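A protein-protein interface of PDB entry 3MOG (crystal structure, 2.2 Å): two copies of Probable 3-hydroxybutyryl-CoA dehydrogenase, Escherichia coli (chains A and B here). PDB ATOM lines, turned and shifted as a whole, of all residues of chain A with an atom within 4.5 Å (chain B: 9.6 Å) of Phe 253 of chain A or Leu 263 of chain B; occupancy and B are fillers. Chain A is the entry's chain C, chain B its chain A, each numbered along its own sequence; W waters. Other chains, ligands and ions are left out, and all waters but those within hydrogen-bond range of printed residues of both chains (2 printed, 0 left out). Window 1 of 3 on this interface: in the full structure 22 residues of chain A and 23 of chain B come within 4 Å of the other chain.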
ATOM      1  N   PRO A 187      14.274 -10.888  -8.446  1.00  0.00           N
ATOM      2  CA  PRO A 187      15.173 -11.953  -7.994  1.00  0.00           C
ATOM      3  C   PRO A 187      15.762 -12.785  -9.132  1.00  0.00           C
ATOM      4  O   PRO A 187      15.008 -13.332  -9.947  1.00  0.00           O
ATOM      5  CB  PRO A 187      14.262 -12.850  -7.157  1.00  0.00           C
ATOM      6  CG  PRO A 187      13.158 -11.962  -6.705  1.00  0.00           C
ATOM      7  CD  PRO A 187      12.960 -10.961  -7.776  1.00  0.00           C
ATOM      8  N   ARG A 193      17.797 -16.520 -12.769  1.00  0.00           N
ATOM      9  CA  ARG A 193      16.408 -16.949 -12.661  1.00  0.00           C
ATOM     10  C   ARG A 193      16.057 -18.030 -13.682  1.00  0.00           C
ATOM     11  O   ARG A 193      15.521 -19.069 -13.318  1.00  0.00           O
ATOM     12  CB  ARG A 193      15.470 -15.746 -12.819  1.00  0.00           C
ATOM     13  CG  ARG A 193      13.995 -16.080 -12.714  1.00  0.00           C
ATOM     14  CD  ARG A 193      13.198 -15.144 -13.580  1.00  0.00           C
ATOM     15  NE  ARG A 193      11.755 -15.301 -13.441  1.00  0.00           N
ATOM     16  CZ  ARG A 193      10.931 -14.331 -13.057  1.00  0.00           C
ATOM     17  NH1 ARG A 193      11.417 -13.152 -12.720  1.00  0.00           N
ATOM     18  NH2 ARG A 193       9.624 -14.553 -12.969  1.00  0.00           N
ATOM     19  N   VAL A 249      16.978 -17.288  -4.713  1.00  0.00           N
ATOM     20  CA  VAL A 249      15.870 -17.066  -5.651  1.00  0.00           C
ATOM     21  C   VAL A 249      14.575 -17.654  -5.063  1.00  0.00           C
ATOM     22  O   VAL A 249      13.535 -16.992  -5.021  1.00  0.00           O
ATOM     23  CB  VAL A 249      16.184 -17.649  -7.056  1.00  0.00           C
ATOM     24  CG1 VAL A 249      15.011 -17.492  -7.976  1.00  0.00           C
ATOM     25  CG2 VAL A 249      17.400 -16.947  -7.663  1.00  0.00           C
ATOM     26  N   PHE A 250      14.671 -18.877  -4.560  1.00  0.00           N
ATOM     27  CA  PHE A 250      13.558 -19.539  -3.884  1.00  0.00           C
ATOM     28  C   PHE A 250      12.909 -18.666  -2.794  1.00  0.00           C
ATOM     29  O   PHE A 250      11.681 -18.494  -2.772  1.00  0.00           O
ATOM     30  CB  PHE A 250      14.059 -20.857  -3.273  1.00  0.00           C
ATOM     31  CG  PHE A 250      13.013 -21.641  -2.514  1.00  0.00           C
ATOM     32  CD1 PHE A 250      11.912 -22.179  -3.169  1.00  0.00           C
ATOM     33  CD2 PHE A 250      13.149 -21.860  -1.147  1.00  0.00           C
ATOM     34  CE1 PHE A 250      10.965 -22.922  -2.491  1.00  0.00           C
ATOM     35  CE2 PHE A 250      12.200 -22.605  -0.447  1.00  0.00           C
ATOM     36  CZ  PHE A 250      11.118 -23.139  -1.107  1.00  0.00           C
ATOM     37  N   ASN A 251      13.739 -18.119  -1.909  1.00  0.00           N
ATOM     38  CA  ASN A 251      13.263 -17.331  -0.773  1.00  0.00           C
ATOM     39  C   ASN A 251      12.774 -15.941  -1.160  1.00  0.00           C
ATOM     40  O   ASN A 251      11.851 -15.435  -0.545  1.00  0.00           O
ATOM     41  CB  ASN A 251      14.351 -17.215   0.301  1.00  0.00           C
ATOM     42  CG  ASN A 251      14.594 -18.530   1.034  1.00  0.00           C
ATOM     43  OD1 ASN A 251      13.652 -19.240   1.408  1.00  0.00           O
ATOM     44  ND2 ASN A 251      15.858 -18.857   1.243  1.00  0.00           N
ATOM     45  N   ALA A 252      13.388 -15.342  -2.185  1.00  0.00           N
ATOM     46  CA  ALA A 252      12.989 -14.019  -2.651  1.00  0.00           C
ATOM     47  C   ALA A 252      11.659 -14.043  -3.402  1.00  0.00           C
ATOM     48  O   ALA A 252      11.048 -12.990  -3.627  1.00  0.00           O
ATOM     49  CB  ALA A 252      14.101 -13.375  -3.504  1.00  0.00           C
ATOM     50  N   PHE A 253      11.224 -15.240  -3.800  1.00  0.00           N
ATOM     51  CA  PHE A 253       9.922 -15.444  -4.441  1.00  0.00           C
ATOM     52  C   PHE A 253       8.937 -16.056  -3.447  1.00  0.00           C
ATOM     53  O   PHE A 253       7.891 -16.633  -3.836  1.00  0.00           O
ATOM     54  CB  PHE A 253      10.037 -16.343  -5.669  1.00  0.00           C
ATOM     55  CG  PHE A 253      10.412 -15.618  -6.951  1.00  0.00           C
ATOM     56  CD1 PHE A 253      11.618 -15.881  -7.576  1.00  0.00           C
ATOM     57  CD2 PHE A 253       9.528 -14.716  -7.558  1.00  0.00           C
ATOM     58  CE1 PHE A 253      11.971 -15.236  -8.788  1.00  0.00           C
ATOM     59  CE2 PHE A 253       9.866 -14.070  -8.747  1.00  0.00           C
ATOM     60  CZ  PHE A 253      11.097 -14.338  -9.370  1.00  0.00           C
ATOM     61  N   TRP A 254       9.272 -15.917  -2.163  1.00  0.00           N
ATOM     62  CA  TRP A 254       8.446 -16.415  -1.068  1.00  0.00           C
ATOM     63  C   TRP A 254       8.115 -17.889  -1.272  1.00  0.00           C
ATOM     64  O   TRP A 254       6.944 -18.297  -1.284  1.00  0.00           O
ATOM     65  CB  TRP A 254       7.181 -15.571  -0.900  1.00  0.00           C
ATOM     66  CG  TRP A 254       7.453 -14.126  -0.584  1.00  0.00           C
ATOM     67  CD1 TRP A 254       7.913 -13.606   0.606  1.00  0.00           C
ATOM     68  CD2 TRP A 254       7.268 -13.008  -1.465  1.00  0.00           C
ATOM     69  NE1 TRP A 254       8.040 -12.244   0.503  1.00  0.00           N
ATOM     70  CE2 TRP A 254       7.652 -11.846  -0.751  1.00  0.00           C
ATOM     71  CE3 TRP A 254       6.832 -12.876  -2.793  1.00  0.00           C
ATOM     72  CZ2 TRP A 254       7.610 -10.568  -1.319  1.00  0.00           C
ATOM     73  CZ3 TRP A 254       6.787 -11.606  -3.359  1.00  0.00           C
ATOM     74  CH2 TRP A 254       7.172 -10.469  -2.620  1.00  0.00           C
ATOM     75  N   GLN A 255       9.153 -18.688  -1.435  1.00  0.00           N
ATOM     76  CA  GLN A 255       9.073 -20.144  -1.543  1.00  0.00           C
ATOM     77  C   GLN A 255       8.279 -20.797  -2.678  1.00  0.00           C
ATOM     78  O   GLN A 255       7.687 -21.818  -2.491  1.00  0.00           O
ATOM     79  CB  GLN A 255       8.649 -20.754  -0.213  1.00  0.00           C
ATOM     80  CG  GLN A 255       9.581 -20.513   0.908  1.00  0.00           C
ATOM     81  CD  GLN A 255       9.421 -19.160   1.512  1.00  0.00           C
ATOM     82  OE1 GLN A 255       8.321 -18.719   1.775  1.00  0.00           O
ATOM     83  NE2 GLN A 255      10.523 -18.500   1.755  1.00  0.00           N
ATOM     84  N   GLU A 256       8.309 -20.196  -3.843  1.00  0.00           N
ATOM     85  CA  GLU A 256       7.797 -20.758  -5.099  1.00  0.00           C
ATOM     86  C   GLU A 256       8.409 -22.121  -5.416  1.00  0.00           C
ATOM     87  O   GLU A 256       9.630 -22.247  -5.484  1.00  0.00           O
ATOM     88  CB  GLU A 256       8.130 -19.819  -6.270  1.00  0.00           C
ATOM     89  CG  GLU A 256       7.200 -18.641  -6.462  1.00  0.00           C
ATOM     90  CD  GLU A 256       5.794 -19.021  -6.920  1.00  0.00           C
ATOM     91  OE1 GLU A 256       5.639 -20.053  -7.621  1.00  0.00           O
ATOM     92  OE2 GLU A 256       4.847 -18.264  -6.585  1.00  0.00           O
ATOM     93  N   PHE A 259      11.170 -23.147  -7.796  1.00  0.00           N
ATOM     94  CA  PHE A 259      12.532 -22.845  -7.372  1.00  0.00           C
ATOM     95  C   PHE A 259      12.971 -23.654  -6.123  1.00  0.00           C
ATOM     96  O   PHE A 259      13.949 -23.314  -5.484  1.00  0.00           O
ATOM     97  CB  PHE A 259      12.721 -21.330  -7.146  1.00  0.00           C
ATOM     98  CG  PHE A 259      12.490 -20.496  -8.376  1.00  0.00           C
ATOM     99  CD1 PHE A 259      11.498 -19.517  -8.391  1.00  0.00           C
ATOM    100  CD2 PHE A 259      13.260 -20.693  -9.528  1.00  0.00           C
ATOM    101  CE1 PHE A 259      11.275 -18.739  -9.530  1.00  0.00           C
ATOM    102  CE2 PHE A 259      13.042 -19.925 -10.676  1.00  0.00           C
ATOM    103  CZ  PHE A 259      12.050 -18.942 -10.676  1.00  0.00           C
ATOM    104  N   SER B 200      -4.668  -8.124  -3.580  1.00  0.00           N
ATOM    105  CA  SER B 200      -3.717  -9.034  -4.237  1.00  0.00           C
ATOM    106  C   SER B 200      -3.955  -9.241  -5.723  1.00  0.00           C
ATOM    107  O   SER B 200      -2.989  -9.312  -6.486  1.00  0.00           O
ATOM    108  CB  SER B 200      -3.590 -10.368  -3.502  1.00  0.00           C
ATOM    109  OG  SER B 200      -4.767 -11.152  -3.589  1.00  0.00           O
ATOM    110  N   TRP B 203      -2.500  -6.189  -7.609  1.00  0.00           N
ATOM    111  CA  TRP B 203      -1.047  -6.266  -7.759  1.00  0.00           C
ATOM    112  C   TRP B 203      -0.630  -7.243  -8.848  1.00  0.00           C
ATOM    113  O   TRP B 203       0.322  -6.985  -9.561  1.00  0.00           O
ATOM    114  CB  TRP B 203      -0.370  -6.643  -6.438  1.00  0.00           C
ATOM    115  CG  TRP B 203      -0.459  -5.580  -5.376  1.00  0.00           C
ATOM    116  CD1 TRP B 203      -1.055  -5.697  -4.164  1.00  0.00           C
ATOM    117  CD2 TRP B 203       0.071  -4.252  -5.435  1.00  0.00           C
ATOM    118  NE1 TRP B 203      -0.936  -4.530  -3.459  1.00  0.00           N
ATOM    119  CE2 TRP B 203      -0.246  -3.625  -4.218  1.00  0.00           C
ATOM    120  CE3 TRP B 203       0.801  -3.537  -6.392  1.00  0.00           C
ATOM    121  CZ2 TRP B 203       0.115  -2.303  -3.935  1.00  0.00           C
ATOM    122  CZ3 TRP B 203       1.156  -2.223  -6.110  1.00  0.00           C
ATOM    123  CH2 TRP B 203       0.818  -1.627  -4.890  1.00  0.00           C
ATOM    124  N   ARG B 204      -1.356  -8.352  -8.978  1.00  0.00           N
ATOM    125  CA  ARG B 204      -1.062  -9.340 -10.016  1.00  0.00           C
ATOM    126  C   ARG B 204      -1.298  -8.795 -11.424  1.00  0.00           C
ATOM    127  O   ARG B 204      -0.542  -9.104 -12.359  1.00  0.00           O
ATOM    128  CB  ARG B 204      -1.887 -10.604  -9.796  1.00  0.00           C
ATOM    129  CG  ARG B 204      -1.206 -11.616  -8.907  1.00  0.00           C
ATOM    130  CD  ARG B 204      -1.974 -12.891  -8.911  1.00  0.00           C
ATOM    131  NE  ARG B 204      -1.822 -13.676 -10.139  1.00  0.00           N
ATOM    132  CZ  ARG B 204      -1.372 -14.930 -10.165  1.00  0.00           C
ATOM    133  NH1 ARG B 204      -1.017 -15.530  -9.035  1.00  0.00           N
ATOM    134  NH2 ARG B 204      -1.288 -15.595 -11.314  1.00  0.00           N
ATOM    135  N   LEU B 206      -1.192  -5.585 -12.260  1.00  0.00           N
ATOM    136  CA  LEU B 206      -0.099  -4.646 -12.472  1.00  0.00           C
ATOM    137  C   LEU B 206       1.191  -5.315 -12.895  1.00  0.00           C
ATOM    138  O   LEU B 206       1.813  -4.890 -13.863  1.00  0.00           O
ATOM    139  CB  LEU B 206       0.158  -3.832 -11.213  1.00  0.00           C
ATOM    140  CG  LEU B 206      -0.552  -2.487 -11.098  1.00  0.00           C
ATOM    141  CD1 LEU B 206      -0.065  -1.804  -9.850  1.00  0.00           C
ATOM    142  CD2 LEU B 206      -0.307  -1.607 -12.339  1.00  0.00           C
ATOM    143  N   GLU B 207       1.597  -6.367 -12.183  1.00  0.00           N
ATOM    144  CA  GLU B 207       2.804  -7.077 -12.578  1.00  0.00           C
ATOM    145  C   GLU B 207       2.760  -7.548 -14.038  1.00  0.00           C
ATOM    146  O   GLU B 207       3.787  -7.514 -14.735  1.00  0.00           O
ATOM    147  CB  GLU B 207       3.081  -8.252 -11.661  1.00  0.00           C
ATOM    148  CG  GLU B 207       4.519  -8.729 -11.751  1.00  0.00           C
ATOM    149  CD  GLU B 207       4.934  -9.586 -10.563  1.00  0.00           C
ATOM    150  OE1 GLU B 207       4.264  -9.520  -9.516  1.00  0.00           O
ATOM    151  OE2 GLU B 207       5.930 -10.319 -10.675  1.00  0.00           O
ATOM    152  N   PHE B 243       1.205  -3.743   3.111  1.00  0.00           N
ATOM    153  CA  PHE B 243       2.155  -4.818   2.821  1.00  0.00           C
ATOM    154  C   PHE B 243       2.397  -5.636   4.081  1.00  0.00           C
ATOM    155  O   PHE B 243       2.393  -6.863   4.024  1.00  0.00           O
ATOM    156  CB  PHE B 243       3.476  -4.224   2.316  1.00  0.00           C
ATOM    157  CG  PHE B 243       4.516  -5.243   1.884  1.00  0.00           C
ATOM    158  CD1 PHE B 243       4.321  -6.041   0.752  1.00  0.00           C
ATOM    159  CD2 PHE B 243       5.722  -5.353   2.574  1.00  0.00           C
ATOM    160  CE1 PHE B 243       5.303  -6.966   0.332  1.00  0.00           C
ATOM    161  CE2 PHE B 243       6.708  -6.264   2.166  1.00  0.00           C
ATOM    162  CZ  PHE B 243       6.493  -7.079   1.036  1.00  0.00           C
ATOM    163  N   THR B 246      -0.525  -7.954   4.746  1.00  0.00           N
ATOM    164  CA  THR B 246      -0.424  -9.019   3.749  1.00  0.00           C
ATOM    165  C   THR B 246       0.629 -10.041   4.169  1.00  0.00           C
ATOM    166  O   THR B 246       0.331 -11.224   4.272  1.00  0.00           O
ATOM    167  CB  THR B 246      -0.123  -8.454   2.345  1.00  0.00           C
ATOM    168  OG1 THR B 246      -1.260  -7.711   1.889  1.00  0.00           O
ATOM    169  CG2 THR B 246       0.174  -9.581   1.352  1.00  0.00           C
ATOM    170  N   CYS B 247       1.841  -9.576   4.460  1.00  0.00           N
ATOM    171  CA  CYS B 247       2.916 -10.465   4.922  1.00  0.00           C
ATOM    172  C   CYS B 247       2.583 -11.199   6.222  1.00  0.00           C
ATOM    173  O   CYS B 247       2.821 -12.404   6.345  1.00  0.00           O
ATOM    174  CB  CYS B 247       4.246  -9.700   5.037  1.00  0.00           C
ATOM    175  SG  CYS B 247       4.913  -9.201   3.403  1.00  0.00           S
ATOM    176  N   PHE B 250       0.088 -13.985   5.569  1.00  0.00           N
ATOM    177  CA  PHE B 250       0.771 -14.986   4.755  1.00  0.00           C
ATOM    178  C   PHE B 250       1.608 -15.888   5.629  1.00  0.00           C
ATOM    179  O   PHE B 250       1.490 -17.120   5.567  1.00  0.00           O
ATOM    180  CB  PHE B 250       1.641 -14.243   3.727  1.00  0.00           C
ATOM    181  CG  PHE B 250       2.556 -15.114   2.901  1.00  0.00           C
ATOM    182  CD1 PHE B 250       2.046 -16.017   1.969  1.00  0.00           C
ATOM    183  CD2 PHE B 250       3.938 -14.945   2.979  1.00  0.00           C
ATOM    184  CE1 PHE B 250       2.904 -16.786   1.165  1.00  0.00           C
ATOM    185  CE2 PHE B 250       4.807 -15.699   2.190  1.00  0.00           C
ATOM    186  CZ  PHE B 250       4.287 -16.625   1.274  1.00  0.00           C
ATOM    187  N   GLN B 255       2.647 -19.584   4.945  1.00  0.00           N
ATOM    188  CA  GLN B 255       2.890 -19.361   3.543  1.00  0.00           C
ATOM    189  C   GLN B 255       1.883 -19.923   2.531  1.00  0.00           C
ATOM    190  O   GLN B 255       2.251 -20.448   1.510  1.00  0.00           O
ATOM    191  CB  GLN B 255       4.268 -19.881   3.200  1.00  0.00           C
ATOM    192  CG  GLN B 255       5.395 -19.111   3.766  1.00  0.00           C
ATOM    193  CD  GLN B 255       5.712 -19.497   5.166  1.00  0.00           C
ATOM    194  OE1 GLN B 255       6.092 -18.668   5.963  1.00  0.00           O
ATOM    195  NE2 GLN B 255       5.550 -20.756   5.480  1.00  0.00           N
ATOM    196  N   ARG B 257      -0.502 -19.794  -0.412  1.00  0.00           N
ATOM    197  CA  ARG B 257      -0.348 -19.043  -1.661  1.00  0.00           C
ATOM    198  C   ARG B 257      -1.468 -18.056  -1.987  1.00  0.00           C
ATOM    199  O   ARG B 257      -1.243 -17.056  -2.678  1.00  0.00           O
ATOM    200  CB  ARG B 257      -0.211 -20.038  -2.800  1.00  0.00           C
ATOM    201  CG  ARG B 257       0.989 -19.803  -3.635  1.00  0.00           C
ATOM    202  CD  ARG B 257       2.209 -20.504  -3.097  1.00  0.00           C
ATOM    203  NE  ARG B 257       3.365 -19.818  -3.650  1.00  0.00           N
ATOM    204  CZ  ARG B 257       4.491 -19.577  -2.997  1.00  0.00           C
ATOM    205  NH1 ARG B 257       4.655 -19.979  -1.740  1.00  0.00           N
ATOM    206  NH2 ARG B 257       5.449 -18.908  -3.615  1.00  0.00           N
ATOM    207  N   LEU B 260      -0.166 -14.752  -0.897  1.00  0.00           N
ATOM    208  CA  LEU B 260       1.183 -14.382  -1.369  1.00  0.00           C
ATOM    209  C   LEU B 260       1.350 -12.865  -1.484  1.00  0.00           C
ATOM    210  O   LEU B 260       0.434 -12.184  -1.953  1.00  0.00           O
ATOM    211  CB  LEU B 260       1.463 -15.036  -2.724  1.00  0.00           C
ATOM    212  CG  LEU B 260       2.899 -15.163  -3.244  1.00  0.00           C
ATOM    213  CD1 LEU B 260       3.685 -16.097  -2.370  1.00  0.00           C
ATOM    214  CD2 LEU B 260       2.921 -15.681  -4.684  1.00  0.00           C
ATOM    215  N   PRO B 261       2.512 -12.333  -1.047  1.00  0.00           N
ATOM    216  CA  PRO B 261       2.803 -10.931  -1.264  1.00  0.00           C
ATOM    217  C   PRO B 261       3.190 -10.710  -2.710  1.00  0.00           C
ATOM    218  O   PRO B 261       3.350 -11.679  -3.462  1.00  0.00           O
ATOM    219  CB  PRO B 261       4.016 -10.660  -0.354  1.00  0.00           C
ATOM    220  CG  PRO B 261       4.045 -11.808   0.623  1.00  0.00           C
ATOM    221  CD  PRO B 261       3.511 -12.965  -0.164  1.00  0.00           C
ATOM    222  N   SER B 262       3.340  -9.441  -3.086  1.00  0.00           N
ATOM    223  CA  SER B 262       3.664  -9.066  -4.456  1.00  0.00           C
ATOM    224  C   SER B 262       5.003  -8.368  -4.473  1.00  0.00           C
ATOM    225  O   SER B 262       5.256  -7.528  -3.613  1.00  0.00           O
ATOM    226  CB  SER B 262       2.607  -8.115  -4.995  1.00  0.00           C
ATOM    227  OG  SER B 262       2.998  -7.561  -6.255  1.00  0.00           O
ATOM    228  N   LEU B 263       5.840  -8.702  -5.459  1.00  0.00           N
ATOM    229  CA  LEU B 263       7.123  -8.017  -5.679  1.00  0.00           C
ATOM    230  C   LEU B 263       6.938  -6.551  -6.022  1.00  0.00           C
ATOM    231  O   LEU B 263       7.812  -5.730  -5.754  1.00  0.00           O
ATOM    232  CB  LEU B 263       7.912  -8.665  -6.830  1.00  0.00           C
ATOM    233  CG  LEU B 263       8.466 -10.078  -6.656  1.00  0.00           C
ATOM    234  CD1 LEU B 263       9.066 -10.521  -8.004  1.00  0.00           C
ATOM    235  CD2 LEU B 263       9.488 -10.168  -5.496  1.00  0.00           C
ATOM    236  N   VAL B 264       5.819  -6.245  -6.666  1.00  0.00           N
ATOM    237  CA  VAL B 264       5.497  -4.879  -7.073  1.00  0.00           C
ATOM    238  C   VAL B 264       5.287  -3.995  -5.841  1.00  0.00           C
ATOM    239  O   VAL B 264       5.883  -2.923  -5.740  1.00  0.00           O
ATOM    240  CB  VAL B 264       4.230  -4.846  -7.954  1.00  0.00           C
ATOM    241  CG1 VAL B 264       3.917  -3.395  -8.438  1.00  0.00           C
ATOM    242  CG2 VAL B 264       4.380  -5.809  -9.140  1.00  0.00           C
ATOM    243  N   GLN B 265       4.448  -4.455  -4.911  1.00  0.00           N
ATOM    244  CA  GLN B 265       4.195  -3.713  -3.676  1.00  0.00           C
ATOM    245  C   GLN B 265       5.460  -3.640  -2.819  1.00  0.00           C
ATOM    246  O   GLN B 265       5.782  -2.577  -2.291  1.00  0.00           O
ATOM    247  CB  GLN B 265       3.042  -4.332  -2.867  1.00  0.00           C
ATOM    248  CG  GLN B 265       2.657  -3.478  -1.662  1.00  0.00           C
ATOM    249  CD  GLN B 265       1.449  -3.951  -0.909  1.00  0.00           C
ATOM    250  OE1 GLN B 265       1.187  -5.146  -0.810  1.00  0.00           O
ATOM    251  NE2 GLN B 265       0.709  -2.999  -0.326  1.00  0.00           N
ATOM    252  N   GLN B 266       6.167  -4.767  -2.695  1.00  0.00           N
ATOM    253  CA  GLN B 266       7.480  -4.823  -2.011  1.00  0.00           C
ATOM    254  C   GLN B 266       8.454  -3.748  -2.501  1.00  0.00           C
ATOM    255  O   GLN B 266       8.986  -2.975  -1.708  1.00  0.00           O
ATOM    256  CB  GLN B 266       8.129  -6.209  -2.149  1.00  0.00           C
ATOM    257  CG  GLN B 266       9.489  -6.295  -1.493  1.00  0.00           C
ATOM    258  CD  GLN B 266       9.968  -7.710  -1.286  1.00  0.00           C
ATOM    259  OE1 GLN B 266       9.987  -8.209  -0.162  1.00  0.00           O
ATOM    260  NE2 GLN B 266      10.371  -8.361  -2.365  1.00  0.00           N
ATOM    261  N   GLU B 267       8.648  -3.689  -3.815  1.00  0.00           N
ATOM    262  CA  GLU B 267       9.501  -2.675  -4.443  1.00  0.00           C
ATOM    263  C   GLU B 267       9.150  -1.225  -4.015  1.00  0.00           C
ATOM    264  O   GLU B 267      10.045  -0.416  -3.751  1.00  0.00           O
ATOM    265  CB  GLU B 267       9.416  -2.831  -5.964  1.00  0.00           C
ATOM    266  CG  GLU B 267      10.362  -1.984  -6.746  1.00  0.00           C
ATOM    267  CD  GLU B 267      11.555  -2.750  -7.293  1.00  0.00           C
ATOM    268  OE1 GLU B 267      12.198  -3.530  -6.538  1.00  0.00           O
ATOM    269  OE2 GLU B 267      11.867  -2.537  -8.486  1.00  0.00           O
ATOM    270  N   LEU B 268       7.859  -0.902  -3.936  1.00  0.00           N
ATOM    271  CA  LEU B 268       7.434   0.429  -3.473  1.00  0.00           C
ATOM    272  C   LEU B 268       7.769   0.674  -1.992  1.00  0.00           C
ATOM    273  O   LEU B 268       8.248   1.750  -1.643  1.00  0.00           O
ATOM    274  CB  LEU B 268       5.937   0.672  -3.739  1.00  0.00           C
ATOM    275  CG  LEU B 268       5.418   0.711  -5.187  1.00  0.00           C
ATOM    276  CD1 LEU B 268       3.908   0.713  -5.164  1.00  0.00           C
ATOM    277  CD2 LEU B 268       5.947   1.892  -6.008  1.00  0.00           C
ATOM    278  N   VAL B 269       7.532  -0.330  -1.140  1.00  0.00           N
ATOM    279  CA  VAL B 269       7.814  -0.225   0.305  1.00  0.00           C
ATOM    280  C   VAL B 269       9.298  -0.028   0.560  1.00  0.00           C
ATOM    281  O   VAL B 269       9.710   0.895   1.262  1.00  0.00           O
ATOM    282  CB  VAL B 269       7.283  -1.447   1.072  1.00  0.00           C
ATOM    283  CG1 VAL B 269       7.778  -1.480   2.537  1.00  0.00           C
ATOM    284  CG2 VAL B 269       5.780  -1.471   1.010  1.00  0.00           C
ATOM    285  N   ILE B 270      10.093  -0.883  -0.073  1.00  0.00           N
ATOM    286  CA  ILE B 270      11.542  -0.831  -0.024  1.00  0.00           C
ATOM    287  C   ILE B 270      12.088   0.481  -0.620  1.00  0.00           C
ATOM    288  O   ILE B 270      13.056   1.052  -0.112  1.00  0.00           O
ATOM    289  CB  ILE B 270      12.113  -2.109  -0.683  1.00  0.00           C
ATOM    290  CG1 ILE B 270      12.308  -3.194   0.377  1.00  0.00           C
ATOM    291  CG2 ILE B 270      13.405  -1.849  -1.427  1.00  0.00           C
ATOM    292  CD1 ILE B 270      12.555  -4.591  -0.194  1.00  0.00           C
ATOM    293  N   GLY B 271      11.435   0.980  -1.659  1.00  0.00           N
ATOM    294  CA  GLY B 271      11.831   2.240  -2.275  1.00  0.00           C
ATOM    295  C   GLY B 271      11.228   3.472  -1.614  1.00  0.00           C
ATOM    296  O   GLY B 271      11.393   4.576  -2.108  1.00  0.00           O
HETATM  297  O   HOH W   1       4.473 -22.220  -5.808  1.00  0.00           O
HETATM  298  O   HOH W   2      11.712 -10.520  -2.752  1.00  0.00           O
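O of Phe 253 of chain A lies within hydrogen-bond range of NH2 of Arg 257 of chain B (3.3 Å). The backbone carbonyl oxygen (O) of Trp 254 of chain A is in hydrogen-bond range of the guanidinium group (NH2) of Arg 257 of chain B (2.8 Å). The guanidinium group (NH2) of Arg 257 of chain B is in salt-bridge range of the side-chain carboxylate (OE2) of Glu 256 of chain A, at 3.1 Å.
OD1 of Asn 251 of chain A sits at hydrogen-bond distance from NE2 of Gln 255 of chain A (3.2 Å). O of Phe 250 of chain B is in hydrogen-bond range of N of Gln 255 of chain B, at 2.8 Å. O of Phe 250 of chain A sits at hydrogen-bond distance from N of Gln 255 of chain A, at 2.9 Å. The backbone NH (N) of Val 264 of chain B sits at hydrogen-bond distance from the side-chain hydroxyl (OG) of Ser 262 of chain B.
Leu 263 of chain B touches Pro 187 of chain A (CD1 to CD, 3.9 Å). Leu 263 of chain B touches Ala 252 of chain A. Phe 253 of chain A touches Leu 263 of chain B (CE2 to CD1, 3.7 Å). Trp 254 of chain A touches Phe 250 of chain B. Trp 254 of chain A touches Leu 260 of chain B (CB to CD1, 3.8 Å). Trp 254 of chain A touches Pro 261 of chain B. Trp 254 of chain A touches Ser 262 of chain B. Trp 254 of chain A touches Leu 263 of chain B. Trp 254 of chain A touches Gln 266 of chain B. Glu 256 of chain A touches Leu 260 of chain B.
Leu 263 of chain B touches four residues of chain A. Pro 187 of chain A touches just one residue of chain B: Leu 263 (3.9 Å). Printed residues of chain A within 4 Å of Phe 250 of chain B: Trp 254. Printed residues of chain B within 4 Å of Glu 256 of chain A: Arg 257 and Leu 260. Thr 246 of chain B touches none of the printed residues of chain A.
Of the 11 printed residues of chain A, 6 touch a printed residue of chain B. Printed residues of chain A that touch a printed residue of chain B: Pro 187, Ala 252, Phe 253, Trp 254, Gln 255 and Glu 256. Hydrophobic or aromatic side chains of chain A that line the printed part of chain B: Pro 187, Phe 253 and Trp 254. Among the printed residues, Asp or Glu carboxylates within 4 Å of a Lys or Arg side-chain nitrogen of the other chain: Glu 256 of chain A with Arg 257 of chain B.
Gln 255 of chain A touches its own counterpart, Gln 255 of chain B. Positions printed for both chains: 250 and 255. Of the 15 pairs that touch across the chains among the printed residues, 1 has its exchanged pair printed and touching as well.
Water W2 lies within hydrogen-bond range of NE2 of Gln 266 of chain B (2.6 Å) and O of Ala 252 of chain A (2.7 Å). Water W1 lies within hydrogen-bond range of OE1 of Glu 256 of chain A (3.1 Å) and NE of Arg 257 of chain B (3.4 Å).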
